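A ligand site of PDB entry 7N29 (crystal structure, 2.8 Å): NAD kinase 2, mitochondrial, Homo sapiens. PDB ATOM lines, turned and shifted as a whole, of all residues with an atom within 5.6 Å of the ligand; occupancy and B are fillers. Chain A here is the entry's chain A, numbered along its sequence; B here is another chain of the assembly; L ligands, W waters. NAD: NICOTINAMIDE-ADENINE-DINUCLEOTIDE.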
ATOM      1  N   ASP A 117       6.907 -14.058 -27.795  1.00  0.00           N
ATOM      2  CA  ASP A 117       6.214 -15.350 -27.756  1.00  0.00           C
ATOM      3  C   ASP A 117       5.375 -15.553 -29.001  1.00  0.00           C
ATOM      4  O   ASP A 117       5.162 -16.696 -29.412  1.00  0.00           O
ATOM      5  CB  ASP A 117       5.318 -15.457 -26.531  1.00  0.00           C
ATOM      6  CG  ASP A 117       6.117 -15.535 -25.242  1.00  0.00           C
ATOM      7  OD1 ASP A 117       7.293 -15.985 -25.309  1.00  0.00           O
ATOM      8  OD2 ASP A 117       5.559 -15.137 -24.179  1.00  0.00           O
ATOM      9  N   GLY A 118       4.834 -14.488 -29.577  1.00  0.00           N
ATOM     10  CA  GLY A 118       4.108 -14.632 -30.825  1.00  0.00           C
ATOM     11  C   GLY A 118       5.006 -15.098 -31.948  1.00  0.00           C
ATOM     12  O   GLY A 118       4.590 -15.877 -32.804  1.00  0.00           O
ATOM     13  N   THR A 119       6.250 -14.627 -31.953  1.00  0.00           N
ATOM     14  CA  THR A 119       7.165 -15.039 -33.004  1.00  0.00           C
ATOM     15  C   THR A 119       7.606 -16.472 -32.768  1.00  0.00           C
ATOM     16  O   THR A 119       7.790 -17.220 -33.726  1.00  0.00           O
ATOM     17  CB  THR A 119       8.349 -14.106 -33.070  1.00  0.00           C
ATOM     18  OG1 THR A 119       9.136 -14.303 -31.898  1.00  0.00           O
ATOM     19  CG2 THR A 119       7.860 -12.664 -33.045  1.00  0.00           C
ATOM     20  N   LEU A 121       5.463 -18.489 -31.685  1.00  0.00           N
ATOM     21  CA  LEU A 121       4.302 -19.220 -32.170  1.00  0.00           C
ATOM     22  C   LEU A 121       4.315 -19.327 -33.688  1.00  0.00           C
ATOM     23  O   LEU A 121       3.956 -20.365 -34.254  1.00  0.00           O
ATOM     24  CB  LEU A 121       3.019 -18.549 -31.703  1.00  0.00           C
ATOM     25  CG  LEU A 121       2.819 -18.606 -30.211  1.00  0.00           C
ATOM     26  CD1 LEU A 121       1.587 -17.806 -29.913  1.00  0.00           C
ATOM     27  CD2 LEU A 121       2.752 -20.055 -29.783  1.00  0.00           C
ATOM     28  N   SER A 144       8.134  -6.475 -24.168  1.00  0.00           N
ATOM     29  CA  SER A 144       7.330  -7.604 -24.601  1.00  0.00           C
ATOM     30  C   SER A 144       7.931  -8.908 -24.090  1.00  0.00           C
ATOM     31  O   SER A 144       8.221  -9.834 -24.844  1.00  0.00           O
ATOM     32  CB  SER A 144       7.172  -7.592 -26.117  1.00  0.00           C
ATOM     33  OG  SER A 144       6.538  -6.393 -26.538  1.00  0.00           O
ATOM     34  N   GLU A 145       8.137  -8.951 -22.777  1.00  0.00           N
ATOM     35  CA  GLU A 145       8.682 -10.107 -22.067  1.00  0.00           C
ATOM     36  C   GLU A 145       7.919 -11.376 -22.419  1.00  0.00           C
ATOM     37  O   GLU A 145       6.713 -11.487 -22.175  1.00  0.00           O
ATOM     38  CB  GLU A 145       8.665  -9.849 -20.567  1.00  0.00           C
ATOM     39  CG  GLU A 145       9.535  -8.689 -20.151  1.00  0.00           C
ATOM     40  CD  GLU A 145       9.404  -8.316 -18.693  1.00  0.00           C
ATOM     41  OE1 GLU A 145       8.615  -8.966 -17.979  1.00  0.00           O
ATOM     42  OE2 GLU A 145      10.094  -7.365 -18.242  1.00  0.00           O
ATOM     43  N   GLY A 146       8.656 -12.356 -22.959  1.00  0.00           N
ATOM     44  CA  GLY A 146       8.113 -13.532 -23.578  1.00  0.00           C
ATOM     45  C   GLY A 146       8.542 -14.840 -22.926  1.00  0.00           C
ATOM     46  O   GLY A 146       9.732 -15.225 -22.969  1.00  0.00           O
ATOM     47  N   HIS A 147       7.569 -15.538 -22.347  1.00  0.00           N
ATOM     48  CA  HIS A 147       7.808 -16.732 -21.550  1.00  0.00           C
ATOM     49  C   HIS A 147       8.327 -17.921 -22.372  1.00  0.00           C
ATOM     50  O   HIS A 147       8.815 -18.897 -21.774  1.00  0.00           O
ATOM     51  CB  HIS A 147       6.500 -17.108 -20.826  1.00  0.00           C
ATOM     52  CG  HIS A 147       5.926 -15.992 -19.997  1.00  0.00           C
ATOM     53  ND1 HIS A 147       5.347 -14.872 -20.550  1.00  0.00           N
ATOM     54  CD2 HIS A 147       5.847 -15.827 -18.648  1.00  0.00           C
ATOM     55  CE1 HIS A 147       4.941 -14.057 -19.589  1.00  0.00           C
ATOM     56  NE2 HIS A 147       5.229 -14.619 -18.422  1.00  0.00           N
ATOM     57  N   LEU A 148       8.309 -17.851 -23.707  1.00  0.00           N
ATOM     58  CA  LEU A 148       8.785 -18.928 -24.575  1.00  0.00           C
ATOM     59  C   LEU A 148      10.174 -18.687 -25.127  1.00  0.00           C
ATOM     60  O   LEU A 148      10.685 -19.524 -25.882  1.00  0.00           O
ATOM     61  CB  LEU A 148       7.823 -19.110 -25.749  1.00  0.00           C
ATOM     62  CG  LEU A 148       6.377 -19.290 -25.284  1.00  0.00           C
ATOM     63  CD1 LEU A 148       5.331 -19.233 -26.423  1.00  0.00           C
ATOM     64  CD2 LEU A 148       6.286 -20.600 -24.497  1.00  0.00           C
ATOM     65  N   HIS A 195      -2.679 -13.015 -39.280  1.00  0.00           N
ATOM     66  CA  HIS A 195      -1.760 -11.877 -39.311  1.00  0.00           C
ATOM     67  C   HIS A 195      -1.573 -11.297 -40.699  1.00  0.00           C
ATOM     68  O   HIS A 195      -0.838 -10.327 -40.840  1.00  0.00           O
ATOM     69  CB  HIS A 195      -0.420 -12.305 -38.694  1.00  0.00           C
ATOM     70  CG  HIS A 195      -0.518 -12.567 -37.221  1.00  0.00           C
ATOM     71  ND1 HIS A 195      -0.331 -11.579 -36.290  1.00  0.00           N
ATOM     72  CD2 HIS A 195      -0.856 -13.680 -36.535  1.00  0.00           C
ATOM     73  CE1 HIS A 195      -0.508 -12.083 -35.080  1.00  0.00           C
ATOM     74  NE2 HIS A 195      -0.853 -13.351 -35.204  1.00  0.00           N
ATOM     75  N   ASN A 232       0.181 -23.298 -27.982  1.00  0.00           N
ATOM     76  CA  ASN A 232      -0.583 -22.707 -26.890  1.00  0.00           C
ATOM     77  C   ASN A 232      -1.946 -23.395 -26.824  1.00  0.00           C
ATOM     78  O   ASN A 232      -2.198 -24.204 -25.932  1.00  0.00           O
ATOM     79  CB  ASN A 232      -0.716 -21.186 -27.058  1.00  0.00           C
ATOM     80  CG  ASN A 232       0.494 -20.430 -26.539  1.00  0.00           C
ATOM     81  OD1 ASN A 232       1.352 -20.961 -25.841  1.00  0.00           O
ATOM     82  ND2 ASN A 232       0.566 -19.155 -26.882  1.00  0.00           N
ATOM     83  N   GLU A 233      -2.815 -23.129 -27.793  1.00  0.00           N
ATOM     84  CA  GLU A 233      -4.145 -23.683 -27.649  1.00  0.00           C
ATOM     85  C   GLU A 233      -4.874 -23.695 -28.981  1.00  0.00           C
ATOM     86  O   GLU A 233      -4.459 -23.021 -29.940  1.00  0.00           O
ATOM     87  CB  GLU A 233      -4.960 -22.903 -26.616  1.00  0.00           C
ATOM     88  CG  GLU A 233      -5.490 -21.606 -27.112  1.00  0.00           C
ATOM     89  CD  GLU A 233      -4.392 -20.608 -27.253  1.00  0.00           C
ATOM     90  OE1 GLU A 233      -3.675 -20.468 -26.230  1.00  0.00           O
ATOM     91  OE2 GLU A 233      -4.234 -20.036 -28.365  1.00  0.00           O
ATOM     92  N   THR A 270       2.163 -25.894 -22.045  1.00  0.00           N
ATOM     93  CA  THR A 270       2.725 -24.626 -22.493  1.00  0.00           C
ATOM     94  C   THR A 270       1.633 -23.571 -22.566  1.00  0.00           C
ATOM     95  O   THR A 270       1.807 -22.445 -22.086  1.00  0.00           O
ATOM     96  CB  THR A 270       3.379 -24.762 -23.862  1.00  0.00           C
ATOM     97  OG1 THR A 270       4.478 -25.673 -23.789  1.00  0.00           O
ATOM     98  CG2 THR A 270       3.844 -23.394 -24.346  1.00  0.00           C
ATOM     99  N   GLY A 271       0.494 -23.939 -23.117  1.00  0.00           N
ATOM    100  CA  GLY A 271      -0.537 -22.948 -23.288  1.00  0.00           C
ATOM    101  C   GLY A 271      -1.292 -22.589 -22.041  1.00  0.00           C
ATOM    102  O   GLY A 271      -2.002 -21.595 -22.052  1.00  0.00           O
ATOM    103  N   LYS A 273      -0.361 -21.206 -19.379  1.00  0.00           N
ATOM    104  CA  LYS A 273       0.004 -19.900 -18.857  1.00  0.00           C
ATOM    105  C   LYS A 273      -0.534 -18.758 -19.704  1.00  0.00           C
ATOM    106  O   LYS A 273      -0.352 -17.588 -19.347  1.00  0.00           O
ATOM    107  CB  LYS A 273       1.535 -19.792 -18.758  1.00  0.00           C
ATOM    108  CG  LYS A 273       2.194 -20.751 -17.755  1.00  0.00           C
ATOM    109  CD  LYS A 273       2.501 -22.142 -18.344  1.00  0.00           C
ATOM    110  CE  LYS A 273       3.265 -23.029 -17.341  1.00  0.00           C
ATOM    111  NZ  LYS A 273       3.564 -24.395 -17.842  1.00  0.00           N
ATOM    112  N   ALA A 274      -1.166 -19.052 -20.825  1.00  0.00           N
ATOM    113  CA  ALA A 274      -1.560 -18.060 -21.802  1.00  0.00           C
ATOM    114  C   ALA A 274      -3.081 -17.791 -21.667  1.00  0.00           C
ATOM    115  O   ALA A 274      -3.520 -17.481 -20.556  1.00  0.00           O
ATOM    116  CB  ALA A 274      -1.092 -18.520 -23.181  1.00  0.00           C
ATOM    117  N   TRP A 275      -3.875 -17.885 -22.737  1.00  0.00           N
ATOM    118  CA  TRP A 275      -5.278 -17.496 -22.694  1.00  0.00           C
ATOM    119  C   TRP A 275      -6.027 -18.262 -21.607  1.00  0.00           C
ATOM    120  O   TRP A 275      -6.785 -17.660 -20.830  1.00  0.00           O
ATOM    121  CB  TRP A 275      -5.919 -17.726 -24.066  1.00  0.00           C
ATOM    122  CG  TRP A 275      -7.187 -16.970 -24.329  1.00  0.00           C
ATOM    123  CD1 TRP A 275      -7.915 -16.212 -23.427  1.00  0.00           C
ATOM    124  CD2 TRP A 275      -7.915 -16.917 -25.565  1.00  0.00           C
ATOM    125  NE1 TRP A 275      -9.034 -15.695 -24.045  1.00  0.00           N
ATOM    126  CE2 TRP A 275      -9.072 -16.117 -25.342  1.00  0.00           C
ATOM    127  CE3 TRP A 275      -7.710 -17.471 -26.830  1.00  0.00           C
ATOM    128  CZ2 TRP A 275      -9.998 -15.862 -26.352  1.00  0.00           C
ATOM    129  CZ3 TRP A 275      -8.647 -17.227 -27.821  1.00  0.00           C
ATOM    130  CH2 TRP A 275      -9.769 -16.418 -27.577  1.00  0.00           C
ATOM    131  N   SER A 276      -5.779 -19.574 -21.512  1.00  0.00           N
ATOM    132  CA  SER A 276      -6.480 -20.375 -20.506  1.00  0.00           C
ATOM    133  C   SER A 276      -6.379 -19.779 -19.103  1.00  0.00           C
ATOM    134  O   SER A 276      -7.355 -19.771 -18.351  1.00  0.00           O
ATOM    135  CB  SER A 276      -5.940 -21.782 -20.495  1.00  0.00           C
ATOM    136  OG  SER A 276      -6.437 -22.438 -19.335  1.00  0.00           O
ATOM    137  N   ASN A 278      -6.039 -16.657 -18.159  1.00  0.00           N
ATOM    138  CA  ASN A 278      -6.896 -15.505 -17.975  1.00  0.00           C
ATOM    139  C   ASN A 278      -8.369 -15.878 -18.114  1.00  0.00           C
ATOM    140  O   ASN A 278      -9.241 -15.185 -17.557  1.00  0.00           O
ATOM    141  CB  ASN A 278      -6.507 -14.413 -18.966  1.00  0.00           C
ATOM    142  CG  ASN A 278      -5.021 -14.053 -18.882  1.00  0.00           C
ATOM    143  OD1 ASN A 278      -4.343 -13.900 -19.903  1.00  0.00           O
ATOM    144  ND2 ASN A 278      -4.496 -13.934 -17.661  1.00  0.00           N
ATOM    145  N   ASP A 368      -3.303 -21.133 -31.878  1.00  0.00           N
ATOM    146  CA  ASP A 368      -2.224 -20.252 -31.377  1.00  0.00           C
ATOM    147  C   ASP A 368      -2.402 -18.803 -31.805  1.00  0.00           C
ATOM    148  O   ASP A 368      -1.450 -18.053 -31.910  1.00  0.00           O
ATOM    149  CB  ASP A 368      -0.834 -20.756 -31.803  1.00  0.00           C
ATOM    150  CG  ASP A 368      -0.434 -22.029 -31.091  1.00  0.00           C
ATOM    151  OD1 ASP A 368      -0.999 -22.311 -30.011  1.00  0.00           O
ATOM    152  OD2 ASP A 368       0.450 -22.750 -31.572  1.00  0.00           O
ATOM    153  N   GLY A 369      -3.648 -18.385 -32.018  1.00  0.00           N
ATOM    154  CA  GLY A 369      -3.945 -17.015 -32.345  1.00  0.00           C
ATOM    155  C   GLY A 369      -3.662 -16.603 -33.774  1.00  0.00           C
ATOM    156  O   GLY A 369      -3.967 -15.473 -34.142  1.00  0.00           O
ATOM    157  N   SER B 242     -10.676 -14.243 -31.349  1.00  0.00           N
ATOM    158  CA  SER B 242      -9.432 -14.759 -30.808  1.00  0.00           C
ATOM    159  C   SER B 242      -8.332 -13.710 -30.692  1.00  0.00           C
ATOM    160  O   SER B 242      -7.213 -14.047 -30.343  1.00  0.00           O
ATOM    161  CB  SER B 242      -8.951 -15.922 -31.674  1.00  0.00           C
ATOM    162  OG  SER B 242      -8.781 -15.504 -33.014  1.00  0.00           O
ATOM    163  N   ARG B 243      -8.628 -12.453 -30.982  1.00  0.00           N
ATOM    164  CA  ARG B 243      -7.651 -11.390 -31.011  1.00  0.00           C
ATOM    165  C   ARG B 243      -7.896 -10.481 -29.812  1.00  0.00           C
ATOM    166  O   ARG B 243      -9.029 -10.039 -29.595  1.00  0.00           O
ATOM    167  CB  ARG B 243      -7.770 -10.623 -32.336  1.00  0.00           C
ATOM    168  CG  ARG B 243      -6.712  -9.589 -32.662  1.00  0.00           C
ATOM    169  CD  ARG B 243      -7.096  -8.837 -33.947  1.00  0.00           C
ATOM    170  NE  ARG B 243      -7.313  -9.721 -35.100  1.00  0.00           N
ATOM    171  CZ  ARG B 243      -7.553  -9.299 -36.350  1.00  0.00           C
ATOM    172  NH1 ARG B 243      -7.634  -7.997 -36.619  1.00  0.00           N
ATOM    173  NH2 ARG B 243      -7.711 -10.169 -37.329  1.00  0.00           N
ATOM    174  N   ALA B 244      -6.872 -10.248 -28.998  1.00  0.00           N
ATOM    175  CA  ALA B 244      -7.063  -9.421 -27.808  1.00  0.00           C
ATOM    176  C   ALA B 244      -7.204  -7.958 -28.193  1.00  0.00           C
ATOM    177  O   ALA B 244      -6.745  -7.496 -29.230  1.00  0.00           O
ATOM    178  CB  ALA B 244      -5.919  -9.591 -26.830  1.00  0.00           C
ATOM    179  N   LYS B 260      -5.385  -4.414 -21.746  1.00  0.00           N
ATOM    180  CA  LYS B 260      -5.322  -5.446 -22.770  1.00  0.00           C
ATOM    181  C   LYS B 260      -6.204  -6.592 -22.281  1.00  0.00           C
ATOM    182  O   LYS B 260      -5.953  -7.148 -21.204  1.00  0.00           O
ATOM    183  CB  LYS B 260      -3.872  -5.892 -22.981  1.00  0.00           C
ATOM    184  CG  LYS B 260      -3.638  -6.901 -24.089  1.00  0.00           C
ATOM    185  CD  LYS B 260      -3.202  -6.220 -25.405  1.00  0.00           C
ATOM    186  CE  LYS B 260      -2.807  -7.257 -26.486  1.00  0.00           C
ATOM    187  NZ  LYS B 260      -1.748  -8.214 -26.052  1.00  0.00           N
ATOM    188  N   SER B 261      -7.240  -6.921 -23.023  1.00  0.00           N
ATOM    189  CA  SER B 261      -8.148  -7.971 -22.574  1.00  0.00           C
ATOM    190  C   SER B 261      -8.889  -8.541 -23.760  1.00  0.00           C
ATOM    191  O   SER B 261      -8.630  -8.170 -24.910  1.00  0.00           O
ATOM    192  CB  SER B 261      -9.155  -7.435 -21.575  1.00  0.00           C
ATOM    193  OG  SER B 261     -10.061  -6.621 -22.281  1.00  0.00           O
ATOM    194  N   SER B 262      -9.815  -9.447 -23.484  1.00  0.00           N
ATOM    195  CA  SER B 262     -10.726  -9.963 -24.507  1.00  0.00           C
ATOM    196  C   SER B 262     -12.026  -9.199 -24.572  1.00  0.00           C
ATOM    197  O   SER B 262     -13.070  -9.797 -24.808  1.00  0.00           O
ATOM    198  CB  SER B 262     -10.999 -11.444 -24.271  1.00  0.00           C
ATOM    199  OG  SER B 262      -9.910 -12.225 -24.723  1.00  0.00           O
ATOM    200  N   ARG B 334     -13.289  -8.195 -19.467  1.00  0.00           N
ATOM    201  CA  ARG B 334     -13.402  -9.606 -19.787  1.00  0.00           C
ATOM    202  C   ARG B 334     -12.021 -10.223 -20.062  1.00  0.00           C
ATOM    203  O   ARG B 334     -11.351  -9.860 -21.038  1.00  0.00           O
ATOM    204  CB  ARG B 334     -14.342  -9.719 -20.968  1.00  0.00           C
ATOM    205  CG  ARG B 334     -14.657 -11.079 -21.380  1.00  0.00           C
ATOM    206  CD  ARG B 334     -15.630 -10.918 -22.490  1.00  0.00           C
ATOM    207  NE  ARG B 334     -16.032 -12.214 -22.976  1.00  0.00           N
ATOM    208  CZ  ARG B 334     -15.931 -12.570 -24.235  1.00  0.00           C
ATOM    209  NH1 ARG B 334     -15.443 -11.711 -25.105  1.00  0.00           N
ATOM    210  NH2 ARG B 334     -16.336 -13.775 -24.599  1.00  0.00           N
ATOM    211  N   GLU B 335     -11.563 -11.105 -19.177  1.00  0.00           N
ATOM    212  CA  GLU B 335     -10.287 -11.822 -19.265  1.00  0.00           C
ATOM    213  C   GLU B 335      -9.116 -10.870 -19.408  1.00  0.00           C
ATOM    214  O   GLU B 335      -8.382 -10.910 -20.412  1.00  0.00           O
ATOM    215  CB  GLU B 335     -10.289 -12.812 -20.430  1.00  0.00           C
ATOM    216  CG  GLU B 335     -11.361 -13.871 -20.324  1.00  0.00           C
ATOM    217  CD  GLU B 335     -11.653 -14.536 -21.652  1.00  0.00           C
ATOM    218  OE1 GLU B 335     -10.962 -14.213 -22.658  1.00  0.00           O
ATOM    219  OE2 GLU B 335     -12.599 -15.352 -21.694  1.00  0.00           O
ATOM    220  N   PRO B 336      -8.871 -10.033 -18.410  1.00  0.00           N
ATOM    221  CA  PRO B 336      -7.743  -9.114 -18.497  1.00  0.00           C
ATOM    222  C   PRO B 336      -6.420  -9.870 -18.544  1.00  0.00           C
ATOM    223  O   PRO B 336      -6.284 -10.966 -17.967  1.00  0.00           O
ATOM    224  CB  PRO B 336      -7.874  -8.287 -17.218  1.00  0.00           C
ATOM    225  CG  PRO B 336      -8.625  -9.154 -16.296  1.00  0.00           C
ATOM    226  CD  PRO B 336      -9.584  -9.897 -17.131  1.00  0.00           C
ATOM    227  N   ILE B 337      -5.448  -9.282 -19.249  1.00  0.00           N
ATOM    228  CA  ILE B 337      -4.091  -9.819 -19.383  1.00  0.00           C
ATOM    229  C   ILE B 337      -3.147  -9.023 -18.486  1.00  0.00           C
ATOM    230  O   ILE B 337      -3.105  -7.791 -18.591  1.00  0.00           O
ATOM    231  CB  ILE B 337      -3.621  -9.749 -20.853  1.00  0.00           C
ATOM    232  CG1 ILE B 337      -4.457 -10.687 -21.725  1.00  0.00           C
ATOM    233  CG2 ILE B 337      -2.142 -10.086 -20.970  1.00  0.00           C
ATOM    234  CD1 ILE B 337      -4.369 -10.367 -23.216  1.00  0.00           C
HETATM  235  PA  NAD L   1       0.076 -10.849 -28.359  1.00  0.00           P
HETATM  236  O1A NAD L   1       1.206 -10.020 -27.862  1.00  0.00           O
HETATM  237  O2A NAD L   1      -0.981 -10.224 -29.212  1.00  0.00           O
HETATM  238  O5B NAD L   1      -0.644 -11.546 -27.084  1.00  0.00           O
HETATM  239  C5B NAD L   1      -0.078 -12.694 -26.384  1.00  0.00           C
HETATM  240  C4B NAD L   1       0.319 -12.316 -24.979  1.00  0.00           C
HETATM  241  O4B NAD L   1       0.402 -13.522 -24.167  1.00  0.00           O
HETATM  242  C3B NAD L   1       1.731 -11.719 -24.851  1.00  0.00           C
HETATM  243  O3B NAD L   1       1.861 -11.055 -23.608  1.00  0.00           O
HETATM  244  C2B NAD L   1       2.596 -12.981 -24.813  1.00  0.00           C
HETATM  245  O2B NAD L   1       3.874 -12.800 -24.257  1.00  0.00           O
HETATM  246  C1B NAD L   1       1.734 -13.881 -23.924  1.00  0.00           C
HETATM  247  N9A NAD L   1       1.889 -15.310 -24.177  1.00  0.00           N
HETATM  248  C8A NAD L   1       1.743 -15.972 -25.368  1.00  0.00           C
HETATM  249  N7A NAD L   1       1.943 -17.260 -25.286  1.00  0.00           N
HETATM  250  C5A NAD L   1       2.243 -17.464 -23.940  1.00  0.00           C
HETATM  251  C6A NAD L   1       2.543 -18.626 -23.210  1.00  0.00           C
HETATM  252  N6A NAD L   1       2.581 -19.846 -23.751  1.00  0.00           N
HETATM  253  N1A NAD L   1       2.796 -18.482 -21.890  1.00  0.00           N
HETATM  254  C2A NAD L   1       2.748 -17.258 -21.358  1.00  0.00           C
HETATM  255  N3A NAD L   1       2.460 -16.099 -21.936  1.00  0.00           N
HETATM  256  C4A NAD L   1       2.214 -16.267 -23.251  1.00  0.00           C
HETATM  257  O3  NAD L   1       0.750 -12.119 -29.102  1.00  0.00           O
HETATM  258  PN  NAD L   1       0.127 -13.255 -30.036  1.00  0.00           P
HETATM  259  O1N NAD L   1       1.165 -13.769 -30.970  1.00  0.00           O
HETATM  260  O2N NAD L   1      -1.103 -12.719 -30.685  1.00  0.00           O
HETATM  261  O5D NAD L   1      -0.252 -14.341 -28.932  1.00  0.00           O
HETATM  262  C5D NAD L   1      -1.100 -15.470 -29.271  1.00  0.00           C
HETATM  263  C4D NAD L   1      -1.690 -16.027 -27.993  1.00  0.00           C
HETATM  264  O4D NAD L   1      -2.314 -14.982 -27.228  1.00  0.00           O
HETATM  265  C3D NAD L   1      -2.767 -17.103 -28.157  1.00  0.00           C
HETATM  266  O3D NAD L   1      -2.190 -18.385 -28.335  1.00  0.00           O
HETATM  267  C2D NAD L   1      -3.560 -16.966 -26.853  1.00  0.00           C
HETATM  268  O2D NAD L   1      -3.184 -17.939 -25.902  1.00  0.00           O
HETATM  269  C1D NAD L   1      -3.237 -15.572 -26.311  1.00  0.00           C
HETATM  270  N1N NAD L   1      -4.454 -14.730 -26.179  1.00  0.00           N
HETATM  271  C2N NAD L   1      -4.856 -14.341 -24.931  1.00  0.00           C
HETATM  272  C3N NAD L   1      -6.034 -13.631 -24.757  1.00  0.00           C
HETATM  273  C7N NAD L   1      -6.418 -13.277 -23.353  1.00  0.00           C
HETATM  274  O7N NAD L   1      -7.484 -12.691 -23.149  1.00  0.00           O
HETATM  275  N7N NAD L   1      -5.532 -13.553 -22.407  1.00  0.00           N
HETATM  276  C4N NAD L   1      -6.786 -13.275 -25.875  1.00  0.00           C
HETATM  277  C5N NAD L   1      -6.373 -13.656 -27.122  1.00  0.00           C
HETATM  278  C6N NAD L   1      -5.209 -14.404 -27.253  1.00  0.00           C
HETATM  279  O   HOH W   1      -0.836 -15.708 -32.835  1.00  0.00           O
HETATM  280  O   HOH W   2      -2.053 -14.645 -22.652  1.00  0.00           O
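Water W1 lies within hydrogen-bond range of O of Asp 368 (2.6 Å), NE2 of His 195 (3.3 Å), O1N of the ligand (3.4 Å) and O of Gly 369 (3.4 Å).
O of Glu 335 of chain B lies close to O7N of the ligand (3.4 Å). CA of Gly 118 touches O1N of the ligand, 3.1 Å away. Leu 121 touches the ligand. O of Glu 145 touches O2B of the ligand, at 3.8 Å. CD2 of Leu 148 touches N6A of the ligand, at 3.9 Å. Lys 273 touches the ligand (CB to N1A, 3.6 Å). Ala 274 touches the ligand. Asp 368 touches the ligand (C to O3D, 3.5 Å). Gly 369 touches the ligand. Ser 242 of chain B touches the ligand (O to C5N, 3.4 Å). CB of Ala 244 of chain B touches C4N of the ligand (3.9 Å). CG1 of Ile 337 of chain B touches N7N of the ligand (3.1 Å). Hydrophobic or aromatic side chains within 4 Å of the ligand: Leu 121, His 147, Leu 148, Ala 274, Trp 275, Ala 244 of chain B and Ile 337 of chain B. Within 4 Å of the ligand: Asp 117, Gly 118, Leu 121, Glu 145, His 147, Leu 148, Asn 232, Glu 233, Thr 270, Lys 273, Ala 274, Trp 275, Asn 278, Asp 368, Gly 369, Ser 242 of chain B, Ala 244 of chain B, Lys 260 of chain B, Ser 262 of chain B, Glu 335 of chain B and Ile 337 of chain B.
OD1 of Asp 368 is in hydrogen-bond range of N of Asn 232 (2.5 Å). The side-chain amide nitrogen (ND2) of Asn 278 lies close to the backbone carbonyl oxygen (O) of Pro 336 of chain B, at 3.5 Å. The side-chain carboxylate (OD2) of Asp 117 lies within hydrogen-bond range of the backbone NH (N) of His 147 (2.7 Å). OD1 of Asp 117 is in hydrogen-bond range of N of Leu 148, at 2.7 Å. OG of Ser 262 of chain B sits at hydrogen-bond distance from OE1 of Glu 335 of chain B (3.1 Å). The backbone NH of Ser 262 of chain B is in hydrogen-bond range of the backbone carbonyl oxygen of Arg 334 of chain B (2.9 Å). N of Ile 337 of chain B is in hydrogen-bond range of O of Lys 260 of chain B. The indole nitrogen (NE1) of Trp 275 lies within hydrogen-bond range of the side-chain carboxylate (OE1) of Glu 335 of chain B (2.8 Å).
O2D of the ligand is in hydrogen-bond range of OE1 of Glu 233. The side-chain amide oxygen of Asn 232 lies within hydrogen-bond range of a nitrogen (N6A) of the ligand (2.7 Å). A nitrogen (N7N) of the ligand sits at hydrogen-bond distance from the side-chain amide oxygen (OD1) of Asn 278, at 2.8 Å. An oxygen (O2B) of the ligand lies within hydrogen-bond range of the side-chain carboxylate (OD2) of Asp 117. The side-chain hydroxyl (OG) of Ser 262 of chain B lies within hydrogen-bond range of an oxygen (O7N) of the ligand (2.9 Å). O of Thr 270 lies within hydrogen-bond range of N6A of the ligand. The backbone NH (N) of Trp 275 lies within hydrogen-bond range of an oxygen (O2D) of the ligand (3.2 Å). An oxygen (O7N) of the ligand lies within hydrogen-bond range of the indole nitrogen (NE1) of Trp 275, at 3.5 Å. ND1 of His 147 sits at hydrogen-bond distance from N3A of the ligand (3.4 Å). The side-chain amino group (NZ) of Lys 260 of chain B is in salt-bridge range of an oxygen (O2A) of the ligand (3.8 Å).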
